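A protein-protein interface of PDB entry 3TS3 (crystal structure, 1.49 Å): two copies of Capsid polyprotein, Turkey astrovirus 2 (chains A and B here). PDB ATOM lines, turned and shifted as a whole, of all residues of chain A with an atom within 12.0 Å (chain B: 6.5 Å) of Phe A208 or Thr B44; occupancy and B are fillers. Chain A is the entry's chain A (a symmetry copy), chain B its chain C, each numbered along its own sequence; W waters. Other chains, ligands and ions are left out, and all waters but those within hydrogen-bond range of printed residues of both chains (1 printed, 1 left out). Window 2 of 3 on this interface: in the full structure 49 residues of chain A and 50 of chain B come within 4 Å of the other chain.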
ATOM      1  N   GLY A  32       9.865  -5.559 -12.323  1.00  0.00           N
ATOM      2  CA  GLY A  32       9.413  -5.013 -11.051  1.00  0.00           C
ATOM      3  C   GLY A  32       8.557  -5.860 -10.137  1.00  0.00           C
ATOM      4  O   GLY A  32       7.806  -5.345  -9.324  1.00  0.00           O
ATOM      5  N   GLY A  90       8.475  -7.781  -2.282  1.00  0.00           N
ATOM      6  CA  GLY A  90       7.564  -8.146  -3.343  1.00  0.00           C
ATOM      7  C   GLY A  90       6.949  -6.958  -4.064  1.00  0.00           C
ATOM      8  O   GLY A  90       6.864  -5.877  -3.526  1.00  0.00           O
ATOM      9  N   GLN A  91       6.405  -7.223  -5.241  1.00  0.00           N
ATOM     10  CA  GLN A  91       5.822  -6.214  -6.110  1.00  0.00           C
ATOM     11  C   GLN A  91       4.806  -5.394  -5.305  1.00  0.00           C
ATOM     12  O   GLN A  91       4.048  -5.936  -4.533  1.00  0.00           O
ATOM     13  CB  GLN A  91       5.095  -6.967  -7.226  1.00  0.00           C
ATOM     14  CG  GLN A  91       4.524  -6.124  -8.333  1.00  0.00           C
ATOM     15  CD  GLN A  91       3.952  -6.982  -9.438  1.00  0.00           C
ATOM     16  OE1 GLN A  91       3.309  -7.984  -9.177  1.00  0.00           O
ATOM     17  NE2 GLN A  91       4.183  -6.587 -10.674  1.00  0.00           N
ATOM     18  N   PRO A  92       4.761  -4.085  -5.520  1.00  0.00           N
ATOM     19  CA  PRO A  92       3.975  -3.229  -4.632  1.00  0.00           C
ATOM     20  C   PRO A  92       2.505  -3.614  -4.539  1.00  0.00           C
ATOM     21  O   PRO A  92       1.974  -3.556  -3.449  1.00  0.00           O
ATOM     22  CB  PRO A  92       4.118  -1.844  -5.270  1.00  0.00           C
ATOM     23  CG  PRO A  92       5.468  -1.869  -5.880  1.00  0.00           C
ATOM     24  CD  PRO A  92       5.665  -3.289  -6.370  1.00  0.00           C
ATOM     25  N   ARG A  93       1.891  -4.051  -5.628  1.00  0.00           N
ATOM     26  CA  ARG A  93       0.462  -4.372  -5.607  1.00  0.00           C
ATOM     27  C   ARG A  93       0.142  -5.490  -4.616  1.00  0.00           C
ATOM     28  O   ARG A  93      -0.968  -5.580  -4.112  1.00  0.00           O
ATOM     29  CB  ARG A  93      -0.044  -4.722  -7.009  1.00  0.00           C
ATOM     30  CG  ARG A  93       0.551  -5.997  -7.571  1.00  0.00           C
ATOM     31  CD  ARG A  93       0.073  -6.307  -8.979  1.00  0.00           C
ATOM     32  NE  ARG A  93       0.674  -7.547  -9.462  1.00  0.00           N
ATOM     33  CZ  ARG A  93       0.235  -8.765  -9.159  1.00  0.00           C
ATOM     34  NH1 ARG A  93      -0.833  -8.908  -8.392  1.00  0.00           N
ATOM     35  NH2 ARG A  93       0.854  -9.835  -9.636  1.00  0.00           N
ATOM     36  N   LEU A  94       1.128  -6.338  -4.362  1.00  0.00           N
ATOM     37  CA  LEU A  94       1.004  -7.458  -3.436  1.00  0.00           C
ATOM     38  C   LEU A  94       0.799  -7.069  -1.975  1.00  0.00           C
ATOM     39  O   LEU A  94       0.142  -7.778  -1.234  1.00  0.00           O
ATOM     40  CB  LEU A  94       2.183  -8.422  -3.567  1.00  0.00           C
ATOM     41  CG  LEU A  94       2.401  -9.034  -4.948  1.00  0.00           C
ATOM     42  CD1 LEU A  94       3.662  -9.881  -4.908  1.00  0.00           C
ATOM     43  CD2 LEU A  94       1.213  -9.886  -5.377  1.00  0.00           C
ATOM     44  N   GLY A  95       1.409  -5.969  -1.559  1.00  0.00           N
ATOM     45  CA  GLY A  95       1.358  -5.556  -0.167  1.00  0.00           C
ATOM     46  C   GLY A  95       1.976  -6.615   0.729  1.00  0.00           C
ATOM     47  O   GLY A  95       1.580  -6.795   1.871  1.00  0.00           O
ATOM     48  N   VAL A  96       2.923  -7.357   0.171  1.00  0.00           N
ATOM     49  CA  VAL A  96       3.559  -8.468   0.870  1.00  0.00           C
ATOM     50  C   VAL A  96       4.846  -8.100   1.636  1.00  0.00           C
ATOM     51  O   VAL A  96       5.254  -8.793   2.551  1.00  0.00           O
ATOM     52  CB  VAL A  96       3.786  -9.660  -0.108  1.00  0.00           C
ATOM     53  CG1 VAL A  96       4.931  -9.391  -1.056  1.00  0.00           C
ATOM     54  CG2 VAL A  96       4.011 -10.930   0.647  1.00  0.00           C
ATOM     55  N   TRP A 188      15.592  -3.436  -8.932  1.00  0.00           N
ATOM     56  CA  TRP A 188      14.360  -4.157  -9.233  1.00  0.00           C
ATOM     57  C   TRP A 188      14.596  -5.092 -10.413  1.00  0.00           C
ATOM     58  O   TRP A 188      15.416  -4.804 -11.265  1.00  0.00           O
ATOM     59  CB  TRP A 188      13.253  -3.164  -9.583  1.00  0.00           C
ATOM     60  CG  TRP A 188      12.742  -2.338  -8.432  1.00  0.00           C
ATOM     61  CD1 TRP A 188      13.272  -1.175  -7.958  1.00  0.00           C
ATOM     62  CD2 TRP A 188      11.574  -2.596  -7.649  1.00  0.00           C
ATOM     63  NE1 TRP A 188      12.516  -0.700  -6.920  1.00  0.00           N
ATOM     64  CE2 TRP A 188      11.466  -1.551  -6.711  1.00  0.00           C
ATOM     65  CE3 TRP A 188      10.607  -3.598  -7.658  1.00  0.00           C
ATOM     66  CZ2 TRP A 188      10.445  -1.495  -5.779  1.00  0.00           C
ATOM     67  CZ3 TRP A 188       9.598  -3.538  -6.739  1.00  0.00           C
ATOM     68  CH2 TRP A 188       9.520  -2.496  -5.810  1.00  0.00           C
ATOM     69  N   HIS A 202       7.345   0.454 -16.898  1.00  0.00           N
ATOM     70  CA  HIS A 202       6.736  -0.646 -16.138  1.00  0.00           C
ATOM     71  C   HIS A 202       6.931  -0.609 -14.632  1.00  0.00           C
ATOM     72  O   HIS A 202       6.092  -1.068 -13.881  1.00  0.00           O
ATOM     73  CB  HIS A 202       7.133  -2.013 -16.694  1.00  0.00           C
ATOM     74  CG  HIS A 202       6.768  -2.204 -18.127  1.00  0.00           C
ATOM     75  ND1 HIS A 202       7.384  -3.130 -18.938  1.00  0.00           N
ATOM     76  CD2 HIS A 202       5.870  -1.561 -18.906  1.00  0.00           C
ATOM     77  CE1 HIS A 202       6.864  -3.064 -20.150  1.00  0.00           C
ATOM     78  NE2 HIS A 202       5.947  -2.115 -20.159  1.00  0.00           N
ATOM     79  N   LEU A 203       8.078  -0.102 -14.211  1.00  0.00           N
ATOM     80  CA  LEU A 203       8.457  -0.148 -12.810  1.00  0.00           C
ATOM     81  C   LEU A 203       7.520   0.639 -11.907  1.00  0.00           C
ATOM     82  O   LEU A 203       7.183   1.767 -12.201  1.00  0.00           O
ATOM     83  CB  LEU A 203       9.877   0.405 -12.653  1.00  0.00           C
ATOM     84  CG  LEU A 203      10.493   0.364 -11.250  1.00  0.00           C
ATOM     85  CD1 LEU A 203      10.500  -1.047 -10.714  1.00  0.00           C
ATOM     86  CD2 LEU A 203      11.893   0.920 -11.264  1.00  0.00           C
ATOM     87  N   ARG A 204       7.125   0.016 -10.802  1.00  0.00           N
ATOM     88  CA  ARG A 204       6.354   0.675  -9.761  1.00  0.00           C
ATOM     89  C   ARG A 204       7.115   0.460  -8.465  1.00  0.00           C
ATOM     90  O   ARG A 204       7.604  -0.627  -8.224  1.00  0.00           O
ATOM     91  CB  ARG A 204       4.953   0.077  -9.632  1.00  0.00           C
ATOM     92  CG  ARG A 204       4.106   0.198 -10.866  1.00  0.00           C
ATOM     93  CD  ARG A 204       3.771   1.648 -11.149  1.00  0.00           C
ATOM     94  NE  ARG A 204       2.947   1.780 -12.344  1.00  0.00           N
ATOM     95  CZ  ARG A 204       3.436   1.982 -13.558  1.00  0.00           C
ATOM     96  NH1 ARG A 204       4.738   2.105 -13.739  1.00  0.00           N
ATOM     97  NH2 ARG A 204       2.619   2.086 -14.592  1.00  0.00           N
ATOM     98  N   THR A 205       7.250   1.504  -7.659  1.00  0.00           N
ATOM     99  CA  THR A 205       7.925   1.382  -6.375  1.00  0.00           C
ATOM    100  C   THR A 205       7.039   1.769  -5.194  1.00  0.00           C
ATOM    101  O   THR A 205       7.472   1.712  -4.054  1.00  0.00           O
ATOM    102  CB  THR A 205       9.225   2.200  -6.348  1.00  0.00           C
ATOM    103  OG1 THR A 205       8.922   3.594  -6.282  1.00  0.00           O
ATOM    104  CG2 THR A 205      10.028   1.933  -7.596  1.00  0.00           C
ATOM    105  N   VAL A 206       5.802   2.161  -5.490  1.00  0.00           N
ATOM    106  CA  VAL A 206       4.836   2.572  -4.480  1.00  0.00           C
ATOM    107  C   VAL A 206       3.524   1.835  -4.719  1.00  0.00           C
ATOM    108  O   VAL A 206       3.111   1.688  -5.853  1.00  0.00           O
ATOM    109  CB  VAL A 206       4.555   4.096  -4.573  1.00  0.00           C
ATOM    110  CG1 VAL A 206       3.428   4.508  -3.636  1.00  0.00           C
ATOM    111  CG2 VAL A 206       5.833   4.899  -4.311  1.00  0.00           C
ATOM    112  N   GLN A 207       2.881   1.381  -3.650  1.00  0.00           N
ATOM    113  CA  GLN A 207       1.587   0.711  -3.752  1.00  0.00           C
ATOM    114  C   GLN A 207       0.471   1.757  -3.773  1.00  0.00           C
ATOM    115  O   GLN A 207       0.472   2.669  -2.973  1.00  0.00           O
ATOM    116  CB  GLN A 207       1.400  -0.232  -2.559  1.00  0.00           C
ATOM    117  CG  GLN A 207       0.043  -0.920  -2.454  1.00  0.00           C
ATOM    118  CD  GLN A 207      -0.113  -1.643  -1.121  1.00  0.00           C
ATOM    119  OE1 GLN A 207       0.474  -1.245  -0.122  1.00  0.00           O
ATOM    120  NE2 GLN A 207      -0.884  -2.712  -1.112  1.00  0.00           N
ATOM    121  N   PHE A 208      -0.471   1.627  -4.699  1.00  0.00           N
ATOM    122  CA  PHE A 208      -1.606   2.536  -4.725  1.00  0.00           C
ATOM    123  C   PHE A 208      -2.887   1.735  -4.645  1.00  0.00           C
ATOM    124  O   PHE A 208      -3.201   1.029  -5.577  1.00  0.00           O
ATOM    125  CB  PHE A 208      -1.615   3.395  -5.992  1.00  0.00           C
ATOM    126  CG  PHE A 208      -2.551   4.566  -5.912  1.00  0.00           C
ATOM    127  CD1 PHE A 208      -2.125   5.772  -5.400  1.00  0.00           C
ATOM    128  CD2 PHE A 208      -3.863   4.449  -6.315  1.00  0.00           C
ATOM    129  CE1 PHE A 208      -2.983   6.837  -5.308  1.00  0.00           C
ATOM    130  CE2 PHE A 208      -4.723   5.518  -6.217  1.00  0.00           C
ATOM    131  CZ  PHE A 208      -4.282   6.703  -5.710  1.00  0.00           C
ATOM    132  N   PRO B  40       6.306   2.063   0.030  1.00  0.00           N
ATOM    133  CA  PRO B  40       5.293   2.911   0.656  1.00  0.00           C
ATOM    134  C   PRO B  40       3.933   2.692   0.020  1.00  0.00           C
ATOM    135  O   PRO B  40       3.845   2.230  -1.099  1.00  0.00           O
ATOM    136  CB  PRO B  40       5.779   4.337   0.362  1.00  0.00           C
ATOM    137  CG  PRO B  40       7.199   4.186  -0.109  1.00  0.00           C
ATOM    138  CD  PRO B  40       7.239   2.851  -0.785  1.00  0.00           C
ATOM    139  N   ALA B  41       2.886   3.037   0.747  1.00  0.00           N
ATOM    140  CA  ALA B  41       1.543   2.952   0.209  1.00  0.00           C
ATOM    141  C   ALA B  41       0.977   4.357   0.085  1.00  0.00           C
ATOM    142  O   ALA B  41       1.222   5.205   0.928  1.00  0.00           O
ATOM    143  CB  ALA B  41       0.661   2.088   1.083  1.00  0.00           C
ATOM    144  N   ALA B  42       0.245   4.578  -0.996  1.00  0.00           N
ATOM    145  CA  ALA B  42      -0.356   5.872  -1.278  1.00  0.00           C
ATOM    146  C   ALA B  42      -1.855   5.752  -1.470  1.00  0.00           C
ATOM    147  O   ALA B  42      -2.356   4.720  -1.886  1.00  0.00           O
ATOM    148  CB  ALA B  42       0.263   6.486  -2.524  1.00  0.00           C
ATOM    149  N   THR B  43      -2.545   6.848  -1.187  1.00  0.00           N
ATOM    150  CA  THR B  43      -3.968   6.974  -1.406  1.00  0.00           C
ATOM    151  C   THR B  43      -4.187   8.261  -2.175  1.00  0.00           C
ATOM    152  O   THR B  43      -3.250   8.968  -2.517  1.00  0.00           O
ATOM    153  CB  THR B  43      -4.784   7.044  -0.114  1.00  0.00           C
ATOM    154  OG1 THR B  43      -4.480   8.258   0.578  1.00  0.00           O
ATOM    155  CG2 THR B  43      -4.500   5.850   0.773  1.00  0.00           C
ATOM    156  N   THR B  44      -5.452   8.548  -2.432  1.00  0.00           N
ATOM    157  CA  THR B  44      -5.842   9.732  -3.165  1.00  0.00           C
ATOM    158  C   THR B  44      -5.477  10.996  -2.403  1.00  0.00           C
ATOM    159  O   THR B  44      -5.448  12.069  -2.976  1.00  0.00           O
ATOM    160  CB  THR B  44      -7.337   9.712  -3.509  1.00  0.00           C
ATOM    161  OG1 THR B  44      -8.089   9.330  -2.354  1.00  0.00           O
ATOM    162  CG2 THR B  44      -7.589   8.716  -4.619  1.00  0.00           C
ATOM    163  N   SER B  45      -5.223  10.870  -1.110  1.00  0.00           N
ATOM    164  CA  SER B  45      -4.843  12.023  -0.313  1.00  0.00           C
ATOM    165  C   SER B  45      -3.332  12.243  -0.244  1.00  0.00           C
ATOM    166  O   SER B  45      -2.881  13.231   0.295  1.00  0.00           O
ATOM    167  CB  SER B  45      -5.404  11.896   1.100  1.00  0.00           C
ATOM    168  OG  SER B  45      -6.811  11.880   1.078  1.00  0.00           O
ATOM    169  N   SER B  46      -2.558  11.300  -0.763  1.00  0.00           N
ATOM    170  CA  SER B  46      -1.101  11.370  -0.696  1.00  0.00           C
ATOM    171  C   SER B  46      -0.431  12.504  -1.453  1.00  0.00           C
ATOM    172  O   SER B  46       0.528  13.080  -0.977  1.00  0.00           O
ATOM    173  CB  SER B  46      -0.492  10.033  -1.112  1.00  0.00           C
ATOM    174  OG  SER B  46      -0.757   9.057  -0.122  1.00  0.00           O
ATOM    175  N   ARG B  47      -0.936  12.806  -2.638  1.00  0.00           N
ATOM    176  CA  ARG B  47      -0.311  13.811  -3.488  1.00  0.00           C
ATOM    177  C   ARG B  47      -0.956  15.182  -3.342  1.00  0.00           C
ATOM    178  O   ARG B  47      -2.140  15.347  -3.572  1.00  0.00           O
ATOM    179  CB  ARG B  47      -0.385  13.362  -4.946  1.00  0.00           C
ATOM    180  CG  ARG B  47       0.368  14.258  -5.927  1.00  0.00           C
ATOM    181  CD  ARG B  47       0.099  13.859  -7.362  1.00  0.00           C
ATOM    182  NE  ARG B  47      -1.304  14.046  -7.696  1.00  0.00           N
ATOM    183  CZ  ARG B  47      -1.816  13.894  -8.906  1.00  0.00           C
ATOM    184  NH1 ARG B  47      -1.045  13.561  -9.923  1.00  0.00           N
ATOM    185  NH2 ARG B  47      -3.108  14.083  -9.100  1.00  0.00           N
ATOM    186  N   ARG B 134      -3.936  17.645   5.656  1.00  0.00           N
ATOM    187  CA  ARG B 134      -3.713  16.306   5.116  1.00  0.00           C
ATOM    188  C   ARG B 134      -2.786  15.465   5.977  1.00  0.00           C
ATOM    189  O   ARG B 134      -2.979  14.270   6.119  1.00  0.00           O
ATOM    190  CB  ARG B 134      -3.166  16.362   3.703  1.00  0.00           C
ATOM    191  CG  ARG B 134      -4.143  16.906   2.728  1.00  0.00           C
ATOM    192  CD  ARG B 134      -4.120  16.095   1.477  1.00  0.00           C
ATOM    193  NE  ARG B 134      -4.928  16.707   0.439  1.00  0.00           N
ATOM    194  CZ  ARG B 134      -4.681  16.571  -0.849  1.00  0.00           C
ATOM    195  NH1 ARG B 134      -3.652  15.842  -1.243  1.00  0.00           N
ATOM    196  NH2 ARG B 134      -5.454  17.163  -1.738  1.00  0.00           N
ATOM    197  N   GLY B 176       2.670  11.207 -10.304  1.00  0.00           N
ATOM    198  CA  GLY B 176       1.589  10.539 -11.002  1.00  0.00           C
ATOM    199  C   GLY B 176       0.372  10.392 -10.109  1.00  0.00           C
ATOM    200  O   GLY B 176       0.491  10.296  -8.909  1.00  0.00           O
ATOM    201  N   ALA B 177      -0.804  10.360 -10.721  1.00  0.00           N
ATOM    202  CA  ALA B 177      -2.054  10.247  -9.988  1.00  0.00           C
ATOM    203  C   ALA B 177      -2.102   8.946  -9.199  1.00  0.00           C
ATOM    204  O   ALA B 177      -2.678   8.893  -8.133  1.00  0.00           O
ATOM    205  CB  ALA B 177      -3.244  10.356 -10.927  1.00  0.00           C
ATOM    206  N   GLN B 178      -1.501   7.903  -9.755  1.00  0.00           N
ATOM    207  CA  GLN B 178      -1.427   6.609  -9.096  1.00  0.00           C
ATOM    208  C   GLN B 178      -0.013   6.309  -8.605  1.00  0.00           C
ATOM    209  O   GLN B 178       0.336   5.166  -8.357  1.00  0.00           O
ATOM    210  CB  GLN B 178      -1.945   5.489  -9.996  1.00  0.00           C
ATOM    211  CG  GLN B 178      -3.442   5.544 -10.260  1.00  0.00           C
ATOM    212  CD  GLN B 178      -3.786   5.910 -11.690  1.00  0.00           C
ATOM    213  OE1 GLN B 178      -3.332   6.924 -12.218  1.00  0.00           O
ATOM    214  NE2 GLN B 178      -4.603   5.076 -12.325  1.00  0.00           N
ATOM    215  N   TYR B 179       0.808   7.346  -8.517  1.00  0.00           N
ATOM    216  CA  TYR B 179       2.185   7.207  -8.050  1.00  0.00           C
ATOM    217  C   TYR B 179       3.024   6.324  -8.966  1.00  0.00           C
ATOM    218  O   TYR B 179       4.033   5.775  -8.565  1.00  0.00           O
ATOM    219  CB  TYR B 179       2.244   6.772  -6.572  1.00  0.00           C
ATOM    220  CG  TYR B 179       2.184   7.973  -5.680  1.00  0.00           C
ATOM    221  CD1 TYR B 179       0.975   8.551  -5.355  1.00  0.00           C
ATOM    222  CD2 TYR B 179       3.338   8.581  -5.235  1.00  0.00           C
ATOM    223  CE1 TYR B 179       0.916   9.683  -4.579  1.00  0.00           C
ATOM    224  CE2 TYR B 179       3.287   9.709  -4.458  1.00  0.00           C
ATOM    225  CZ  TYR B 179       2.071  10.257  -4.141  1.00  0.00           C
ATOM    226  OH  TYR B 179       2.018  11.387  -3.376  1.00  0.00           O
HETATM  227  O   HOH W   1       5.868   3.860  -8.485  1.00  0.00           O
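The backbone carbonyl oxygen (O) of Pro B40 lies within hydrogen-bond range of the backbone NH (N) of Gln A207, 2.9 Å away.
The backbone carbonyl oxygen of Gln A207 sits at hydrogen-bond distance from the backbone NH of Ala B42, at 2.8 Å.
N of Ser B45 lies close to OG1 of Thr B43.
The backbone NH of Thr B43 is in hydrogen-bond range of the side-chain hydroxyl of Ser B46 (3.0 Å).
The backbone carbonyl oxygen of Ser B46 sits at hydrogen-bond distance from the side-chain hydroxyl of Tyr B179, at 3.3 Å.
The backbone NH of Arg B47 lies within hydrogen-bond range of the side-chain hydroxyl of Tyr B179 (3.4 Å).
O of Thr A205 touches CD of Pro B40, at 3.5 Å.
Pro B40 touches Val A206.
Val A206 touches Ala B42 (CG1 to CB, 3.9 Å).
CB of Tyr B179 touches CG1 of Val A206, at 3.9 Å.
Gln A207 touches Ala B41 (O to CA, 3.4 Å).
Phe A208 touches Ala B42 (CA to O, 3.7 Å).
CE1 of Phe A208 touches O of Thr B43, at 3.5 Å.
CZ of Phe A208 touches N of Thr B44, 3.9 Å away.
Ala B177 touches Phe A208 (O to CE1, 3.5 Å).
CB of Phe A208 touches O of Gln B178, at 3.5 Å.
Of chain B, only Ala B42, Thr B43, Thr B44, Ala B177 and Gln B178 come within 4 Å of Phe A208.
Of chain A, only Phe A208 comes within 4 Å of Thr B44.
Ala B41 touches one residue of chain A.
No residue of chain A comes within 4 Å of Ser B45.
No residue of chain A comes within 4 Å of Ser B46.
Of chain A, only Phe A208 comes within 4 Å of Ala B177.
Of the printed residues of chain A, Gln B178 touches Phe A208.
Of the printed residues of chain B, Gln A207 touches Pro B40 (2.9 Å), Ala B41 (3.4 Å) and Ala B42 (2.8 Å).
Of the printed residues of chain B, Val A206 touches Pro B40 (3.4 Å), Ala B42 (3.9 Å) and Tyr B179 (3.9 Å).
Of the printed residues of chain B, Thr A205 touches Pro B40 (3.5 Å).
Of the printed residues of chain A, Pro B40 touches Thr A205, Val A206 and Gln A207.
The nearest residue of chain B that does not touch Phe A208 is Tyr B179 (4.2 Å).
Printed residues of chain A that touch a printed residue of chain B: Thr A205, Val A206, Gln A207 and Phe A208.
Along chain A the printed residues that touch a printed residue of chain B span positions 205 to 208.
Of the 13 printed residues of chain B, 8 touch a printed residue of chain A.
Printed residues of chain B that touch a printed residue of chain A: Pro B40, Ala B41, Ala B42, Thr B43, Thr B44, Ala B177, Gln B178 and Tyr B179.
Among the printed residues, 12 pairs touch across the chains.
Among the printed residues, no Asp or Glu carboxylate lies within 4 Å of a Lys or Arg side-chain nitrogen of the other chain.
No position is printed for both chains.
Of the 12 pairs that touch across the chains among the printed residues, none has its exchanged pair printed and touching as well.
Water W1 lies within hydrogen-bond range of O of Tyr B179 (2.7 Å), N of Thr A205 (2.9 Å) and N of Val A206 (3.4 Å).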
